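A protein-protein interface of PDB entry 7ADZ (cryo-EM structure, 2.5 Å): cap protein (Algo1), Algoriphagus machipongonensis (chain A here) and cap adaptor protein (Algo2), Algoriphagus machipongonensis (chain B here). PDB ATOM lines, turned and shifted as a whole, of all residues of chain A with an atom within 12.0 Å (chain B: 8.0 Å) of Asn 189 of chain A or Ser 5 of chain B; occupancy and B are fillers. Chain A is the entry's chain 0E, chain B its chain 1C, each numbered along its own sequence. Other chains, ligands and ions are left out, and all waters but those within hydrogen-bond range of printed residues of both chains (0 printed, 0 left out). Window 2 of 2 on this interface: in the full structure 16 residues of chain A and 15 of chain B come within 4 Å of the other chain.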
ATOM      1  N   THR A  73      20.252  -7.009 -27.281  1.00  0.00           N
ATOM      2  CA  THR A  73      19.999  -8.436 -27.470  1.00  0.00           C
ATOM      3  C   THR A  73      21.033  -8.995 -28.449  1.00  0.00           C
ATOM      4  O   THR A  73      20.710  -9.704 -29.401  1.00  0.00           O
ATOM      5  CB  THR A  73      18.576  -8.708 -27.965  1.00  0.00           C
ATOM      6  OG1 THR A  73      18.335  -7.976 -29.174  1.00  0.00           O
ATOM      7  CG2 THR A  73      17.537  -8.327 -26.916  1.00  0.00           C
ATOM      8  N   GLU A 184      26.350 -12.378 -32.599  1.00  0.00           N
ATOM      9  CA  GLU A 184      25.170 -13.236 -32.568  1.00  0.00           C
ATOM     10  C   GLU A 184      24.095 -12.585 -31.702  1.00  0.00           C
ATOM     11  O   GLU A 184      24.357 -11.630 -30.970  1.00  0.00           O
ATOM     12  CB  GLU A 184      25.534 -14.635 -32.042  1.00  0.00           C
ATOM     13  CG  GLU A 184      24.634 -15.791 -32.491  1.00  0.00           C
ATOM     14  CD  GLU A 184      24.530 -15.931 -33.999  1.00  0.00           C
ATOM     15  OE1 GLU A 184      23.440 -15.668 -34.548  1.00  0.00           O
ATOM     16  OE2 GLU A 184      25.537 -16.310 -34.635  1.00  0.00           O
ATOM     17  N   GLY A 185      22.872 -13.102 -31.800  1.00  0.00           N
ATOM     18  CA  GLY A 185      21.770 -12.639 -30.971  1.00  0.00           C
ATOM     19  C   GLY A 185      21.517 -13.561 -29.787  1.00  0.00           C
ATOM     20  O   GLY A 185      21.815 -14.750 -29.836  1.00  0.00           O
ATOM     21  N   VAL A 186      20.955 -12.989 -28.719  1.00  0.00           N
ATOM     22  CA  VAL A 186      20.783 -13.730 -27.470  1.00  0.00           C
ATOM     23  C   VAL A 186      19.523 -14.593 -27.510  1.00  0.00           C
ATOM     24  O   VAL A 186      18.716 -14.544 -28.443  1.00  0.00           O
ATOM     25  CB  VAL A 186      20.758 -12.772 -26.266  1.00  0.00           C
ATOM     26  CG1 VAL A 186      21.958 -11.863 -26.297  1.00  0.00           C
ATOM     27  CG2 VAL A 186      19.473 -11.964 -26.252  1.00  0.00           C
ATOM     28  N   ILE A 187      19.367 -15.404 -26.464  1.00  0.00           N
ATOM     29  CA  ILE A 187      18.247 -16.330 -26.333  1.00  0.00           C
ATOM     30  C   ILE A 187      16.979 -15.551 -26.004  1.00  0.00           C
ATOM     31  O   ILE A 187      16.939 -14.782 -25.036  1.00  0.00           O
ATOM     32  CB  ILE A 187      18.548 -17.382 -25.254  1.00  0.00           C
ATOM     33  CG1 ILE A 187      19.714 -18.264 -25.691  1.00  0.00           C
ATOM     34  CG2 ILE A 187      17.322 -18.223 -24.944  1.00  0.00           C
ATOM     35  CD1 ILE A 187      20.177 -19.242 -24.642  1.00  0.00           C
ATOM     36  N   THR A 188      15.929 -15.743 -26.813  1.00  0.00           N
ATOM     37  CA  THR A 188      14.633 -15.121 -26.555  1.00  0.00           C
ATOM     38  C   THR A 188      13.441 -16.073 -26.588  1.00  0.00           C
ATOM     39  O   THR A 188      12.344 -15.650 -26.215  1.00  0.00           O
ATOM     40  CB  THR A 188      14.364 -13.975 -27.550  1.00  0.00           C
ATOM     41  OG1 THR A 188      14.491 -14.448 -28.895  1.00  0.00           O
ATOM     42  CG2 THR A 188      15.307 -12.798 -27.333  1.00  0.00           C
ATOM     43  N   ASN A 189      13.603 -17.326 -27.014  1.00  0.00           N
ATOM     44  CA  ASN A 189      12.510 -18.297 -27.043  1.00  0.00           C
ATOM     45  C   ASN A 189      12.995 -19.633 -26.500  1.00  0.00           C
ATOM     46  O   ASN A 189      14.053 -20.119 -26.907  1.00  0.00           O
ATOM     47  CB  ASN A 189      11.964 -18.493 -28.462  1.00  0.00           C
ATOM     48  CG  ASN A 189      11.554 -17.197 -29.122  1.00  0.00           C
ATOM     49  OD1 ASN A 189      10.466 -16.687 -28.885  1.00  0.00           O
ATOM     50  ND2 ASN A 189      12.421 -16.668 -29.972  1.00  0.00           N
ATOM     51  N   ILE A 190      12.224 -20.230 -25.592  1.00  0.00           N
ATOM     52  CA  ILE A 190      12.563 -21.503 -24.964  1.00  0.00           C
ATOM     53  C   ILE A 190      11.412 -22.478 -25.178  1.00  0.00           C
ATOM     54  O   ILE A 190      10.252 -22.142 -24.919  1.00  0.00           O
ATOM     55  CB  ILE A 190      12.871 -21.330 -23.462  1.00  0.00           C
ATOM     56  CG1 ILE A 190      13.991 -20.309 -23.256  1.00  0.00           C
ATOM     57  CG2 ILE A 190      13.270 -22.655 -22.836  1.00  0.00           C
ATOM     58  CD1 ILE A 190      14.178 -19.854 -21.843  1.00  0.00           C
ATOM     59  N   HIS A 191      11.731 -23.680 -25.655  1.00  0.00           N
ATOM     60  CA  HIS A 191      10.757 -24.733 -25.914  1.00  0.00           C
ATOM     61  C   HIS A 191      11.185 -26.000 -25.190  1.00  0.00           C
ATOM     62  O   HIS A 191      12.359 -26.376 -25.238  1.00  0.00           O
ATOM     63  CB  HIS A 191      10.626 -25.017 -27.415  1.00  0.00           C
ATOM     64  CG  HIS A 191      10.391 -23.798 -28.249  1.00  0.00           C
ATOM     65  ND1 HIS A 191       9.156 -23.481 -28.766  1.00  0.00           N
ATOM     66  CD2 HIS A 191      11.235 -22.829 -28.672  1.00  0.00           C
ATOM     67  CE1 HIS A 191       9.248 -22.364 -29.465  1.00  0.00           C
ATOM     68  NE2 HIS A 191      10.500 -21.948 -29.423  1.00  0.00           N
ATOM     69  N   ARG A 192      10.239 -26.659 -24.521  1.00  0.00           N
ATOM     70  CA  ARG A 192      10.510 -27.869 -23.755  1.00  0.00           C
ATOM     71  C   ARG A 192       9.559 -28.979 -24.180  1.00  0.00           C
ATOM     72  O   ARG A 192       8.345 -28.770 -24.243  1.00  0.00           O
ATOM     73  CB  ARG A 192      10.390 -27.608 -22.249  1.00  0.00           C
ATOM     74  CG  ARG A 192      11.468 -26.684 -21.694  1.00  0.00           C
ATOM     75  CD  ARG A 192      11.439 -26.575 -20.178  1.00  0.00           C
ATOM     76  NE  ARG A 192      10.265 -25.871 -19.669  1.00  0.00           N
ATOM     77  CZ  ARG A 192      10.182 -24.553 -19.520  1.00  0.00           C
ATOM     78  NH1 ARG A 192      11.200 -23.778 -19.850  1.00  0.00           N
ATOM     79  NH2 ARG A 192       9.073 -24.007 -19.050  1.00  0.00           N
ATOM     80  N   ASN A 193      10.113 -30.155 -24.463  1.00  0.00           N
ATOM     81  CA  ASN A 193       9.350 -31.320 -24.896  1.00  0.00           C
ATOM     82  C   ASN A 193       9.580 -32.473 -23.930  1.00  0.00           C
ATOM     83  O   ASN A 193      10.723 -32.773 -23.579  1.00  0.00           O
ATOM     84  CB  ASN A 193       9.742 -31.740 -26.311  1.00  0.00           C
ATOM     85  CG  ASN A 193       9.320 -30.733 -27.347  1.00  0.00           C
ATOM     86  OD1 ASN A 193      10.150 -30.036 -27.928  1.00  0.00           O
ATOM     87  ND2 ASN A 193       8.023 -30.660 -27.603  1.00  0.00           N
ATOM     88  N   TYR A 194       8.497 -33.114 -23.510  1.00  0.00           N
ATOM     89  CA  TYR A 194       8.533 -34.185 -22.525  1.00  0.00           C
ATOM     90  C   TYR A 194       7.947 -35.451 -23.129  1.00  0.00           C
ATOM     91  O   TYR A 194       6.977 -35.393 -23.888  1.00  0.00           O
ATOM     92  CB  TYR A 194       7.750 -33.808 -21.261  1.00  0.00           C
ATOM     93  CG  TYR A 194       8.337 -32.663 -20.464  1.00  0.00           C
ATOM     94  CD1 TYR A 194       9.168 -32.903 -19.380  1.00  0.00           C
ATOM     95  CD2 TYR A 194       8.042 -31.345 -20.782  1.00  0.00           C
ATOM     96  CE1 TYR A 194       9.699 -31.863 -18.647  1.00  0.00           C
ATOM     97  CE2 TYR A 194       8.572 -30.298 -20.058  1.00  0.00           C
ATOM     98  CZ  TYR A 194       9.398 -30.563 -18.993  1.00  0.00           C
ATOM     99  OH  TYR A 194       9.923 -29.526 -18.267  1.00  0.00           O
ATOM    100  N   VAL B   3       5.892 -27.399 -24.168  1.00  0.00           N
ATOM    101  CA  VAL B   3       5.867 -26.170 -23.403  1.00  0.00           C
ATOM    102  C   VAL B   3       6.657 -25.116 -24.156  1.00  0.00           C
ATOM    103  O   VAL B   3       7.750 -25.405 -24.639  1.00  0.00           O
ATOM    104  CB  VAL B   3       6.459 -26.399 -21.999  1.00  0.00           C
ATOM    105  CG1 VAL B   3       6.427 -25.107 -21.197  1.00  0.00           C
ATOM    106  CG2 VAL B   3       5.679 -27.513 -21.281  1.00  0.00           C
ATOM    107  N   SER B   4       6.138 -23.901 -24.252  1.00  0.00           N
ATOM    108  CA  SER B   4       6.851 -22.844 -24.952  1.00  0.00           C
ATOM    109  C   SER B   4       6.716 -21.505 -24.249  1.00  0.00           C
ATOM    110  O   SER B   4       5.830 -21.306 -23.417  1.00  0.00           O
ATOM    111  CB  SER B   4       6.338 -22.732 -26.366  1.00  0.00           C
ATOM    112  OG  SER B   4       4.998 -22.333 -26.378  1.00  0.00           O
ATOM    113  N   SER B   5       7.623 -20.591 -24.578  1.00  0.00           N
ATOM    114  CA  SER B   5       7.644 -19.252 -24.015  1.00  0.00           C
ATOM    115  C   SER B   5       8.339 -18.285 -24.956  1.00  0.00           C
ATOM    116  O   SER B   5       9.013 -18.697 -25.899  1.00  0.00           O
ATOM    117  CB  SER B   5       8.341 -19.272 -22.677  1.00  0.00           C
ATOM    118  OG  SER B   5       9.691 -19.582 -22.822  1.00  0.00           O
ATOM    119  N   SER B   6       8.160 -16.997 -24.701  1.00  0.00           N
ATOM    120  CA  SER B   6       8.752 -15.921 -25.479  1.00  0.00           C
ATOM    121  C   SER B   6       8.886 -14.690 -24.615  1.00  0.00           C
ATOM    122  O   SER B   6       7.966 -14.367 -23.863  1.00  0.00           O
ATOM    123  CB  SER B   6       7.877 -15.604 -26.659  1.00  0.00           C
ATOM    124  OG  SER B   6       8.412 -14.559 -27.395  1.00  0.00           O
ATOM    125  N   PHE B   7      10.030 -14.009 -24.696  1.00  0.00           N
ATOM    126  CA  PHE B   7      10.249 -12.835 -23.858  1.00  0.00           C
ATOM    127  C   PHE B   7      10.629 -11.618 -24.679  1.00  0.00           C
ATOM    128  O   PHE B   7      11.364 -11.738 -25.662  1.00  0.00           O
ATOM    129  CB  PHE B   7      11.366 -13.146 -22.876  1.00  0.00           C
ATOM    130  CG  PHE B   7      11.060 -14.339 -22.040  1.00  0.00           C
ATOM    131  CD1 PHE B   7      11.437 -15.589 -22.487  1.00  0.00           C
ATOM    132  CD2 PHE B   7      10.402 -14.251 -20.849  1.00  0.00           C
ATOM    133  CE1 PHE B   7      11.154 -16.705 -21.775  1.00  0.00           C
ATOM    134  CE2 PHE B   7      10.122 -15.391 -20.135  1.00  0.00           C
ATOM    135  CZ  PHE B   7      10.497 -16.606 -20.600  1.00  0.00           C
ATOM    136  N   ARG B   8      10.187 -10.442 -24.229  1.00  0.00           N
ATOM    137  CA  ARG B   8      10.496  -9.175 -24.890  1.00  0.00           C
ATOM    138  C   ARG B   8      10.871  -8.065 -23.910  1.00  0.00           C
ATOM    139  O   ARG B   8      10.457  -8.079 -22.750  1.00  0.00           O
ATOM    140  CB  ARG B   8       9.307  -8.722 -25.724  1.00  0.00           C
ATOM    141  CG  ARG B   8       8.914  -9.668 -26.867  1.00  0.00           C
ATOM    142  CD  ARG B   8       9.919  -9.695 -27.951  1.00  0.00           C
ATOM    143  NE  ARG B   8       9.495 -10.513 -29.050  1.00  0.00           N
ATOM    144  CZ  ARG B   8       9.690 -11.845 -29.185  1.00  0.00           C
ATOM    145  NH1 ARG B   8      10.326 -12.558 -28.273  1.00  0.00           N
ATOM    146  NH2 ARG B   8       9.230 -12.439 -30.277  1.00  0.00           N
ATOM    147  N   LYS B  80       7.545 -11.829 -20.029  1.00  0.00           N
ATOM    148  CA  LYS B  80       6.966 -12.903 -20.840  1.00  0.00           C
ATOM    149  C   LYS B  80       5.712 -12.420 -21.575  1.00  0.00           C
ATOM    150  O   LYS B  80       4.809 -11.837 -20.956  1.00  0.00           O
ATOM    151  CB  LYS B  80       6.614 -14.117 -19.986  1.00  0.00           C
ATOM    152  CG  LYS B  80       6.099 -15.313 -20.777  1.00  0.00           C
ATOM    153  CD  LYS B  80       5.870 -16.529 -19.898  1.00  0.00           C
ATOM    154  CE  LYS B  80       5.218 -17.648 -20.686  1.00  0.00           C
ATOM    155  NZ  LYS B  80       5.062 -18.886 -19.884  1.00  0.00           N
ATOM    156  N   VAL B  81       5.614 -12.755 -22.859  1.00  0.00           N
ATOM    157  CA  VAL B  81       4.463 -12.375 -23.684  1.00  0.00           C
ATOM    158  C   VAL B  81       3.775 -13.590 -24.269  1.00  0.00           C
ATOM    159  O   VAL B  81       4.312 -14.697 -24.235  1.00  0.00           O
ATOM    160  CB  VAL B  81       4.863 -11.422 -24.840  1.00  0.00           C
ATOM    161  CG1 VAL B  81       5.451 -10.129 -24.283  1.00  0.00           C
ATOM    162  CG2 VAL B  81       5.851 -12.109 -25.778  1.00  0.00           C
ATOM    163  N   GLU B  82       2.566 -13.389 -24.770  1.00  0.00           N
ATOM    164  CA  GLU B  82       1.824 -14.472 -25.390  1.00  0.00           C
ATOM    165  C   GLU B  82       2.457 -14.946 -26.684  1.00  0.00           C
ATOM    166  O   GLU B  82       2.914 -14.145 -27.504  1.00  0.00           O
ATOM    167  CB  GLU B  82       0.379 -14.075 -25.663  1.00  0.00           C
ATOM    168  CG  GLU B  82      -0.471 -13.902 -24.431  1.00  0.00           C
ATOM    169  CD  GLU B  82      -1.921 -13.675 -24.758  1.00  0.00           C
ATOM    170  OE1 GLU B  82      -2.240 -13.570 -25.918  1.00  0.00           O
ATOM    171  OE2 GLU B  82      -2.713 -13.635 -23.856  1.00  0.00           O
ATOM    172  N   SER B  83       2.445 -16.252 -26.885  1.00  0.00           N
ATOM    173  CA  SER B  83       2.980 -16.815 -28.103  1.00  0.00           C
ATOM    174  C   SER B  83       2.233 -16.282 -29.303  1.00  0.00           C
ATOM    175  O   SER B  83       1.010 -16.148 -29.283  1.00  0.00           O
ATOM    176  CB  SER B  83       2.911 -18.317 -28.086  1.00  0.00           C
ATOM    177  OG  SER B  83       3.363 -18.834 -29.302  1.00  0.00           O
ATOM    178  N   GLY B  84       2.973 -15.979 -30.356  1.00  0.00           N
ATOM    179  CA  GLY B  84       2.407 -15.467 -31.590  1.00  0.00           C
ATOM    180  C   GLY B  84       2.435 -13.943 -31.688  1.00  0.00           C
ATOM    181  O   GLY B  84       2.221 -13.396 -32.770  1.00  0.00           O
ATOM    182  N   THR B  85       2.719 -13.240 -30.589  1.00  0.00           N
ATOM    183  CA  THR B  85       2.757 -11.784 -30.684  1.00  0.00           C
ATOM    184  C   THR B  85       3.972 -11.126 -30.090  1.00  0.00           C
ATOM    185  O   THR B  85       4.876 -11.760 -29.552  1.00  0.00           O
ATOM    186  CB  THR B  85       1.520 -11.123 -30.085  1.00  0.00           C
ATOM    187  OG1 THR B  85       1.540  -9.720 -30.430  1.00  0.00           O
ATOM    188  CG2 THR B  85       1.489 -11.275 -28.607  1.00  0.00           C
ATOM    189  N   GLU B  86       3.977  -9.809 -30.209  1.00  0.00           N
ATOM    190  CA  GLU B  86       5.053  -8.973 -29.714  1.00  0.00           C
ATOM    191  C   GLU B  86       4.670  -8.084 -28.545  1.00  0.00           C
ATOM    192  O   GLU B  86       5.538  -7.616 -27.812  1.00  0.00           O
ATOM    193  CB  GLU B  86       5.556  -8.087 -30.853  1.00  0.00           C
ATOM    194  CG  GLU B  86       6.109  -8.855 -32.041  1.00  0.00           C
ATOM    195  CD  GLU B  86       7.342  -9.569 -31.671  1.00  0.00           C
ATOM    196  OE1 GLU B  86       8.112  -8.997 -30.952  1.00  0.00           O
ATOM    197  OE2 GLU B  86       7.530 -10.691 -32.074  1.00  0.00           O
ATOM    198  N   PHE B  90       1.813 -11.818 -21.039  1.00  0.00           N
ATOM    199  CA  PHE B  90       1.207 -13.098 -20.735  1.00  0.00           C
ATOM    200  C   PHE B  90       0.143 -12.906 -19.647  1.00  0.00           C
ATOM    201  O   PHE B  90      -1.001 -13.331 -19.779  1.00  0.00           O
ATOM    202  CB  PHE B  90       2.287 -14.087 -20.344  1.00  0.00           C
ATOM    203  CG  PHE B  90       1.791 -15.419 -20.068  1.00  0.00           C
ATOM    204  CD1 PHE B  90       1.502 -16.260 -21.115  1.00  0.00           C
ATOM    205  CD2 PHE B  90       1.600 -15.853 -18.787  1.00  0.00           C
ATOM    206  CE1 PHE B  90       1.027 -17.517 -20.885  1.00  0.00           C
ATOM    207  CE2 PHE B  90       1.124 -17.108 -18.551  1.00  0.00           C
ATOM    208  CZ  PHE B  90       0.835 -17.943 -19.603  1.00  0.00           C
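Ser 6 of chain B touches Thr 188 of chain A.
Asn 189 of chain A touches Ser 5 of chain B (CA to O, 3.7 Å).
O of Ile 190 of chain A touches CA of Ser 4 of chain B, 3.5 Å away.
His 191 of chain A touches Val 3 of chain B (CA to O, 3.3 Å).
His 191 of chain A touches Ser 4 of chain B.
O of Ser 6 of chain B is in hydrogen-bond range of N of Val 81 of chain B (3.0 Å).
OG of Ser 6 of chain B lies within hydrogen-bond range of NH1 of Arg 8 of chain B, at 2.9 Å.
The side-chain hydroxyl of Thr 188 of chain A lies within hydrogen-bond range of the side-chain amide nitrogen of Asn 189 of chain A, 3.2 Å away.
N of Arg 192 of chain A lies within hydrogen-bond range of O of Val 3 of chain B, at 2.8 Å.
The side-chain amide oxygen (OD1) of Asn 189 of chain A lies within hydrogen-bond range of the side-chain hydroxyl (OG) of Ser 6 of chain B, at 3.3 Å.
O of Ile 190 of chain A sits at hydrogen-bond distance from N of Ser 5 of chain B (3.1 Å).
The backbone NH (N) of Phe 7 of chain B sits at hydrogen-bond distance from the backbone carbonyl oxygen (O) of Thr 188 of chain A (3.2 Å).
Of the 14 printed residues of chain B, 5 touch a printed residue of chain A.
Hydrophobic or aromatic side chains of chain B within 4 Å of the printed part of chain A: Val 3 and Phe 7.
Hydrophobic or aromatic side chains of chain A within 4 Å of the printed part of chain B: Ile 190 and His 191.
Among the printed residues, 9 pairs touch across the chains.
Printed residues of chain B within 4 Å of Thr 188 of chain A: Ser 6 and Phe 7.
Of the printed residues of chain B, Ile 190 of chain A touches Ser 4 and Ser 5.
Of the printed residues of chain B, Arg 192 of chain A touches Val 3 (2.8 Å).
Of chain A, only His 191 and Arg 192 come within 4 Å of Val 3 of chain B.
Ser 4 of chain B touches two residues of chain A.
Ser 5 of chain B touches just these residues of chain A: Asn 189 (3.7 Å) and Ile 190 (3.1 Å).
Of chain A, only Thr 188 and Asn 189 come within 4 Å of Ser 6 of chain B.
Of chain A, only Thr 188 comes within 4 Å of Phe 7 of chain B.
Thr 85 of chain B touches none of the printed residues of chain A.
The nearest printed residue of chain B that does not touch Ile 190 of chain A is Val 3 of chain B (4.1 Å).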
